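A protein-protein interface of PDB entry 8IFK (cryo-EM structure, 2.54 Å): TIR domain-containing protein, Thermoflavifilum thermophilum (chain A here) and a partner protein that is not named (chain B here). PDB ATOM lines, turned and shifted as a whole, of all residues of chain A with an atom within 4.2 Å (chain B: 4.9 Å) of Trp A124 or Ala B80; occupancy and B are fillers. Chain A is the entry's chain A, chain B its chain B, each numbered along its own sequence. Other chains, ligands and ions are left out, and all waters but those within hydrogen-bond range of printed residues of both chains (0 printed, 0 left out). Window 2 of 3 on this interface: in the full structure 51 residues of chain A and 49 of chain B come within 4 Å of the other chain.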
ATOM      1  N   PHE A  17      -8.133  23.527  -5.349  1.00  0.00           N
ATOM      2  CA  PHE A  17      -7.352  24.255  -6.342  1.00  0.00           C
ATOM      3  C   PHE A  17      -7.395  25.751  -6.093  1.00  0.00           C
ATOM      4  O   PHE A  17      -6.381  26.440  -6.242  1.00  0.00           O
ATOM      5  CB  PHE A  17      -7.847  23.959  -7.756  1.00  0.00           C
ATOM      6  CG  PHE A  17      -7.283  24.895  -8.788  1.00  0.00           C
ATOM      7  CD1 PHE A  17      -6.013  24.697  -9.296  1.00  0.00           C
ATOM      8  CD2 PHE A  17      -8.015  25.984  -9.233  1.00  0.00           C
ATOM      9  CE1 PHE A  17      -5.486  25.560 -10.233  1.00  0.00           C
ATOM     10  CE2 PHE A  17      -7.491  26.851 -10.172  1.00  0.00           C
ATOM     11  CZ  PHE A  17      -6.224  26.638 -10.672  1.00  0.00           C
ATOM     12  N   TRP A  20      -5.127  26.595  -3.159  1.00  0.00           N
ATOM     13  CA  TRP A  20      -3.723  26.460  -3.530  1.00  0.00           C
ATOM     14  C   TRP A  20      -3.278  27.624  -4.404  1.00  0.00           C
ATOM     15  O   TRP A  20      -2.263  28.271  -4.124  1.00  0.00           O
ATOM     16  CB  TRP A  20      -3.495  25.128  -4.245  1.00  0.00           C
ATOM     17  CG  TRP A  20      -2.124  24.989  -4.835  1.00  0.00           C
ATOM     18  CD1 TRP A  20      -1.002  24.544  -4.200  1.00  0.00           C
ATOM     19  CD2 TRP A  20      -1.731  25.292  -6.179  1.00  0.00           C
ATOM     20  NE1 TRP A  20       0.066  24.554  -5.065  1.00  0.00           N
ATOM     21  CE2 TRP A  20      -0.356  25.010  -6.286  1.00  0.00           C
ATOM     22  CE3 TRP A  20      -2.409  25.777  -7.301  1.00  0.00           C
ATOM     23  CZ2 TRP A  20       0.355  25.195  -7.469  1.00  0.00           C
ATOM     24  CZ3 TRP A  20      -1.702  25.961  -8.474  1.00  0.00           C
ATOM     25  CH2 TRP A  20      -0.335  25.671  -8.549  1.00  0.00           C
ATOM     26  N   LYS A  24      -0.784  30.605  -3.245  1.00  0.00           N
ATOM     27  CA  LYS A  24       0.463  30.670  -3.998  1.00  0.00           C
ATOM     28  C   LYS A  24       0.668  32.052  -4.603  1.00  0.00           C
ATOM     29  O   LYS A  24       1.774  32.601  -4.554  1.00  0.00           O
ATOM     30  CB  LYS A  24       0.464  29.602  -5.093  1.00  0.00           C
ATOM     31  CG  LYS A  24       1.738  28.778  -5.168  1.00  0.00           C
ATOM     32  CD  LYS A  24       1.770  27.710  -4.089  1.00  0.00           C
ATOM     33  CE  LYS A  24       3.034  26.873  -4.181  1.00  0.00           C
ATOM     34  NZ  LYS A  24       3.298  26.421  -5.576  1.00  0.00           N
ATOM     35  N   PHE A 120      -4.576  23.891 -16.223  1.00  0.00           N
ATOM     36  CA  PHE A 120      -3.903  23.195 -15.138  1.00  0.00           C
ATOM     37  C   PHE A 120      -4.170  21.697 -15.169  1.00  0.00           C
ATOM     38  O   PHE A 120      -3.837  20.997 -14.208  1.00  0.00           O
ATOM     39  CB  PHE A 120      -4.329  23.765 -13.781  1.00  0.00           C
ATOM     40  CG  PHE A 120      -3.927  25.201 -13.554  1.00  0.00           C
ATOM     41  CD1 PHE A 120      -4.427  26.221 -14.348  1.00  0.00           C
ATOM     42  CD2 PHE A 120      -3.056  25.527 -12.529  1.00  0.00           C
ATOM     43  CE1 PHE A 120      -4.059  27.533 -14.129  1.00  0.00           C
ATOM     44  CE2 PHE A 120      -2.688  26.839 -12.302  1.00  0.00           C
ATOM     45  CZ  PHE A 120      -3.188  27.842 -13.105  1.00  0.00           C
ATOM     46  N   SER A 123      -0.760  19.649 -15.260  1.00  0.00           N
ATOM     47  CA  SER A 123      -0.034  19.866 -14.018  1.00  0.00           C
ATOM     48  C   SER A 123      -0.377  21.248 -13.486  1.00  0.00           C
ATOM     49  O   SER A 123      -0.555  22.195 -14.256  1.00  0.00           O
ATOM     50  CB  SER A 123       1.480  19.730 -14.220  1.00  0.00           C
ATOM     51  OG  SER A 123       2.191  20.266 -13.118  1.00  0.00           O
ATOM     52  N   TRP A 124      -0.466  21.352 -12.163  1.00  0.00           N
ATOM     53  CA  TRP A 124      -0.709  22.638 -11.525  1.00  0.00           C
ATOM     54  C   TRP A 124       0.516  23.534 -11.511  1.00  0.00           C
ATOM     55  O   TRP A 124       0.364  24.758 -11.516  1.00  0.00           O
ATOM     56  CB  TRP A 124      -1.199  22.444 -10.091  1.00  0.00           C
ATOM     57  CG  TRP A 124      -2.631  22.069 -10.005  1.00  0.00           C
ATOM     58  CD1 TRP A 124      -3.473  21.797 -11.041  1.00  0.00           C
ATOM     59  CD2 TRP A 124      -3.402  21.928  -8.813  1.00  0.00           C
ATOM     60  NE1 TRP A 124      -4.724  21.492 -10.567  1.00  0.00           N
ATOM     61  CE2 TRP A 124      -4.706  21.568  -9.199  1.00  0.00           C
ATOM     62  CE3 TRP A 124      -3.117  22.071  -7.454  1.00  0.00           C
ATOM     63  CZ2 TRP A 124      -5.719  21.340  -8.275  1.00  0.00           C
ATOM     64  CZ3 TRP A 124      -4.122  21.855  -6.543  1.00  0.00           C
ATOM     65  CH2 TRP A 124      -5.406  21.489  -6.954  1.00  0.00           C
ATOM     66  N   ALA A 125       1.719  22.967 -11.487  1.00  0.00           N
ATOM     67  CA  ALA A 125       2.923  23.780 -11.584  1.00  0.00           C
ATOM     68  C   ALA A 125       3.082  24.374 -12.978  1.00  0.00           C
ATOM     69  O   ALA A 125       3.416  25.552 -13.117  1.00  0.00           O
ATOM     70  CB  ALA A 125       4.151  22.951 -11.213  1.00  0.00           C
ATOM     71  N   LYS A 126       2.837  23.571 -14.017  1.00  0.00           N
ATOM     72  CA  LYS A 126       2.863  24.098 -15.377  1.00  0.00           C
ATOM     73  C   LYS A 126       1.792  25.161 -15.574  1.00  0.00           C
ATOM     74  O   LYS A 126       2.052  26.209 -16.175  1.00  0.00           O
ATOM     75  CB  LYS A 126       2.681  22.965 -16.386  1.00  0.00           C
ATOM     76  CG  LYS A 126       3.786  21.923 -16.364  1.00  0.00           C
ATOM     77  CD  LYS A 126       3.468  20.775 -17.309  1.00  0.00           C
ATOM     78  CE  LYS A 126       4.569  19.728 -17.303  1.00  0.00           C
ATOM     79  NZ  LYS A 126       4.246  18.586 -18.201  1.00  0.00           N
ATOM     80  N   GLY A 127       0.582  24.912 -15.069  1.00  0.00           N
ATOM     81  CA  GLY A 127      -0.474  25.904 -15.186  1.00  0.00           C
ATOM     82  C   GLY A 127      -0.160  27.180 -14.430  1.00  0.00           C
ATOM     83  O   GLY A 127      -0.426  28.282 -14.913  1.00  0.00           O
ATOM     84  N   LEU A 128       0.408  27.049 -13.229  1.00  0.00           N
ATOM     85  CA  LEU A 128       0.792  28.224 -12.458  1.00  0.00           C
ATOM     86  C   LEU A 128       1.899  29.003 -13.157  1.00  0.00           C
ATOM     87  O   LEU A 128       1.897  30.235 -13.143  1.00  0.00           O
ATOM     88  CB  LEU A 128       1.227  27.812 -11.052  1.00  0.00           C
ATOM     89  CG  LEU A 128       1.774  28.927 -10.158  1.00  0.00           C
ATOM     90  CD1 LEU A 128       0.710  29.984  -9.904  1.00  0.00           C
ATOM     91  CD2 LEU A 128       2.294  28.361  -8.848  1.00  0.00           C
ATOM     92  N   ALA B  28       2.758  22.174   0.403  1.00  0.00           N
ATOM     93  CA  ALA B  28       1.956  22.684  -0.702  1.00  0.00           C
ATOM     94  C   ALA B  28       1.960  24.207  -0.751  1.00  0.00           C
ATOM     95  O   ALA B  28       1.861  24.790  -1.838  1.00  0.00           O
ATOM     96  CB  ALA B  28       0.525  22.160  -0.601  1.00  0.00           C
ATOM     97  N   PRO B  63      -2.638  16.429 -10.078  1.00  0.00           N
ATOM     98  CA  PRO B  63      -3.162  16.448  -8.706  1.00  0.00           C
ATOM     99  C   PRO B  63      -3.912  15.167  -8.373  1.00  0.00           C
ATOM    100  O   PRO B  63      -4.595  14.584  -9.219  1.00  0.00           O
ATOM    101  CB  PRO B  63      -4.098  17.662  -8.700  1.00  0.00           C
ATOM    102  CG  PRO B  63      -3.643  18.496  -9.837  1.00  0.00           C
ATOM    103  CD  PRO B  63      -3.162  17.546 -10.879  1.00  0.00           C
ATOM    104  N   TYR B  65      -6.423  13.467  -5.230  1.00  0.00           N
ATOM    105  CA  TYR B  65      -7.281  13.805  -4.107  1.00  0.00           C
ATOM    106  C   TYR B  65      -7.530  12.582  -3.235  1.00  0.00           C
ATOM    107  O   TYR B  65      -7.457  11.440  -3.696  1.00  0.00           O
ATOM    108  CB  TYR B  65      -8.622  14.362  -4.596  1.00  0.00           C
ATOM    109  CG  TYR B  65      -8.537  15.744  -5.199  1.00  0.00           C
ATOM    110  CD1 TYR B  65      -8.289  15.916  -6.554  1.00  0.00           C
ATOM    111  CD2 TYR B  65      -8.703  16.876  -4.415  1.00  0.00           C
ATOM    112  CE1 TYR B  65      -8.210  17.176  -7.110  1.00  0.00           C
ATOM    113  CE2 TYR B  65      -8.626  18.141  -4.963  1.00  0.00           C
ATOM    114  CZ  TYR B  65      -8.380  18.286  -6.310  1.00  0.00           C
ATOM    115  OH  TYR B  65      -8.302  19.544  -6.858  1.00  0.00           O
ATOM    116  N   MET B  74      -5.049  16.935   0.186  1.00  0.00           N
ATOM    117  CA  MET B  74      -4.858  16.351  -1.129  1.00  0.00           C
ATOM    118  C   MET B  74      -3.507  16.754  -1.710  1.00  0.00           C
ATOM    119  O   MET B  74      -2.842  17.675  -1.230  1.00  0.00           O
ATOM    120  CB  MET B  74      -5.987  16.776  -2.065  1.00  0.00           C
ATOM    121  CG  MET B  74      -5.953  18.250  -2.393  1.00  0.00           C
ATOM    122  SD  MET B  74      -5.285  18.647  -4.009  1.00  0.00           S
ATOM    123  CE  MET B  74      -4.608  20.255  -3.634  1.00  0.00           C
ATOM    124  N   PRO B  76      -1.368  18.395  -4.532  1.00  0.00           N
ATOM    125  CA  PRO B  76      -1.449  19.289  -5.700  1.00  0.00           C
ATOM    126  C   PRO B  76      -0.682  18.792  -6.913  1.00  0.00           C
ATOM    127  O   PRO B  76      -0.919  19.293  -8.019  1.00  0.00           O
ATOM    128  CB  PRO B  76      -0.851  20.603  -5.175  1.00  0.00           C
ATOM    129  CG  PRO B  76      -0.994  20.520  -3.690  1.00  0.00           C
ATOM    130  CD  PRO B  76      -0.793  19.074  -3.361  1.00  0.00           C
ATOM    131  N   GLY B  77       0.223  17.833  -6.746  1.00  0.00           N
ATOM    132  CA  GLY B  77       1.133  17.447  -7.806  1.00  0.00           C
ATOM    133  C   GLY B  77       2.563  17.617  -7.338  1.00  0.00           C
ATOM    134  O   GLY B  77       2.832  18.472  -6.491  1.00  0.00           O
ATOM    135  N   PHE B  78       3.489  16.812  -7.864  1.00  0.00           N
ATOM    136  CA  PHE B  78       4.846  16.817  -7.325  1.00  0.00           C
ATOM    137  C   PHE B  78       5.537  18.153  -7.565  1.00  0.00           C
ATOM    138  O   PHE B  78       6.148  18.719  -6.653  1.00  0.00           O
ATOM    139  CB  PHE B  78       5.670  15.678  -7.924  1.00  0.00           C
ATOM    140  CG  PHE B  78       7.031  15.546  -7.306  1.00  0.00           C
ATOM    141  CD1 PHE B  78       7.215  14.779  -6.169  1.00  0.00           C
ATOM    142  CD2 PHE B  78       8.120  16.212  -7.840  1.00  0.00           C
ATOM    143  CE1 PHE B  78       8.459  14.664  -5.588  1.00  0.00           C
ATOM    144  CE2 PHE B  78       9.365  16.105  -7.260  1.00  0.00           C
ATOM    145  CZ  PHE B  78       9.535  15.329  -6.134  1.00  0.00           C
ATOM    146  N   GLU B  79       5.472  18.664  -8.796  1.00  0.00           N
ATOM    147  CA  GLU B  79       6.139  19.926  -9.095  1.00  0.00           C
ATOM    148  C   GLU B  79       5.441  21.097  -8.415  1.00  0.00           C
ATOM    149  O   GLU B  79       6.095  22.062  -8.004  1.00  0.00           O
ATOM    150  CB  GLU B  79       6.207  20.146 -10.604  1.00  0.00           C
ATOM    151  CG  GLU B  79       7.208  21.213 -11.011  1.00  0.00           C
ATOM    152  CD  GLU B  79       7.342  21.350 -12.513  1.00  0.00           C
ATOM    153  OE1 GLU B  79       8.461  21.634 -12.986  1.00  0.00           O
ATOM    154  OE2 GLU B  79       6.326  21.177 -13.219  1.00  0.00           O
ATOM    155  N   ALA B  80       4.113  21.032  -8.289  1.00  0.00           N
ATOM    156  CA  ALA B  80       3.376  22.108  -7.638  1.00  0.00           C
ATOM    157  C   ALA B  80       3.729  22.221  -6.161  1.00  0.00           C
ATOM    158  O   ALA B  80       3.487  23.262  -5.542  1.00  0.00           O
ATOM    159  CB  ALA B  80       1.872  21.893  -7.809  1.00  0.00           C
ATOM    160  N   VAL B  81       4.295  21.165  -5.581  1.00  0.00           N
ATOM    161  CA  VAL B  81       4.650  21.155  -4.167  1.00  0.00           C
ATOM    162  C   VAL B  81       6.138  21.422  -3.992  1.00  0.00           C
ATOM    163  O   VAL B  81       6.535  22.372  -3.309  1.00  0.00           O
ATOM    164  CB  VAL B  81       4.264  19.816  -3.514  1.00  0.00           C
ATOM    165  CG1 VAL B  81       4.817  19.746  -2.107  1.00  0.00           C
ATOM    166  CG2 VAL B  81       2.759  19.650  -3.503  1.00  0.00           C
ATOM    167  N   PHE B  82       6.969  20.586  -4.609  1.00  0.00           N
ATOM    168  CA  PHE B  82       8.400  20.568  -4.350  1.00  0.00           C
ATOM    169  C   PHE B  82       9.200  21.454  -5.294  1.00  0.00           C
ATOM    170  O   PHE B  82      10.417  21.570  -5.125  1.00  0.00           O
ATOM    171  CB  PHE B  82       8.916  19.128  -4.417  1.00  0.00           C
ATOM    172  CG  PHE B  82       8.327  18.233  -3.367  1.00  0.00           C
ATOM    173  CD1 PHE B  82       8.763  18.299  -2.055  1.00  0.00           C
ATOM    174  CD2 PHE B  82       7.321  17.340  -3.687  1.00  0.00           C
ATOM    175  CE1 PHE B  82       8.217  17.479  -1.087  1.00  0.00           C
ATOM    176  CE2 PHE B  82       6.772  16.522  -2.723  1.00  0.00           C
ATOM    177  CZ  PHE B  82       7.221  16.590  -1.424  1.00  0.00           C
ATOM    178  N   GLY B  83       8.554  22.082  -6.273  1.00  0.00           N
ATOM    179  CA  GLY B  83       9.256  22.980  -7.167  1.00  0.00           C
ATOM    180  C   GLY B  83      10.317  22.331  -8.024  1.00  0.00           C
ATOM    181  O   GLY B  83      11.238  23.016  -8.477  1.00  0.00           O
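The side-chain amino group (NZ) of Lys A24 lies within hydrogen-bond range of the backbone carbonyl oxygen (O) of Ala B80, 3.2 Å away.
Of chain B, only Pro B63, Tyr B65, Met B74, Pro B76 and Ala B80 come within 4 Å of Trp A124.
Of the printed residues of chain B, Ala A125 touches Glu B79 (3.4 Å) and Ala B80 (3.5 Å).
Of the printed residues of chain A, Ala B28 touches Trp A20 and Lys A24.
Of the printed residues of chain A, Tyr B65 touches Trp A124.
Of the printed residues of chain A, Met B74 touches Trp A124.
Phe B78 touches none of the printed residues of chain A.
Of chain A, only Trp A20 (3.6 Å), Lys A24 (3.2 Å), Trp A124 (3.9 Å) and Ala A125 (3.5 Å) come within 4 Å of Ala B80.
The nearest printed residue of chain A that does not touch Ala B80 is Ser A123 (5.3 Å).
The nearest printed residue of chain A that does not touch Tyr B65 is Phe A17 (4.3 Å).
Among the printed residues, pairs that only touch across the chains: Trp A20 with Ala B28, Trp A20 with Ala B80, Lys A24 with Ala B28, Trp A124 with Pro B63, Trp A124 with Tyr B65, Trp A124 with Met B74, Trp A124 with Pro B76, Trp A124 with Ala B80, Ala A125 with Glu B79 and Ala A125 with Ala B80.
Hydrophobic or aromatic side chains of chain A that line the printed part of chain B: Trp A20, Trp A124 and Ala A125.
Of the 12 printed residues of chain B, 7 touch a printed residue of chain A.
Among the printed residues, no Asp or Glu carboxylate lies within 4 Å of a Lys or Arg side-chain nitrogen of the other chain.
OG of Ser A123 is in hydrogen-bond range of N of Ala A125 (3.2 Å).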
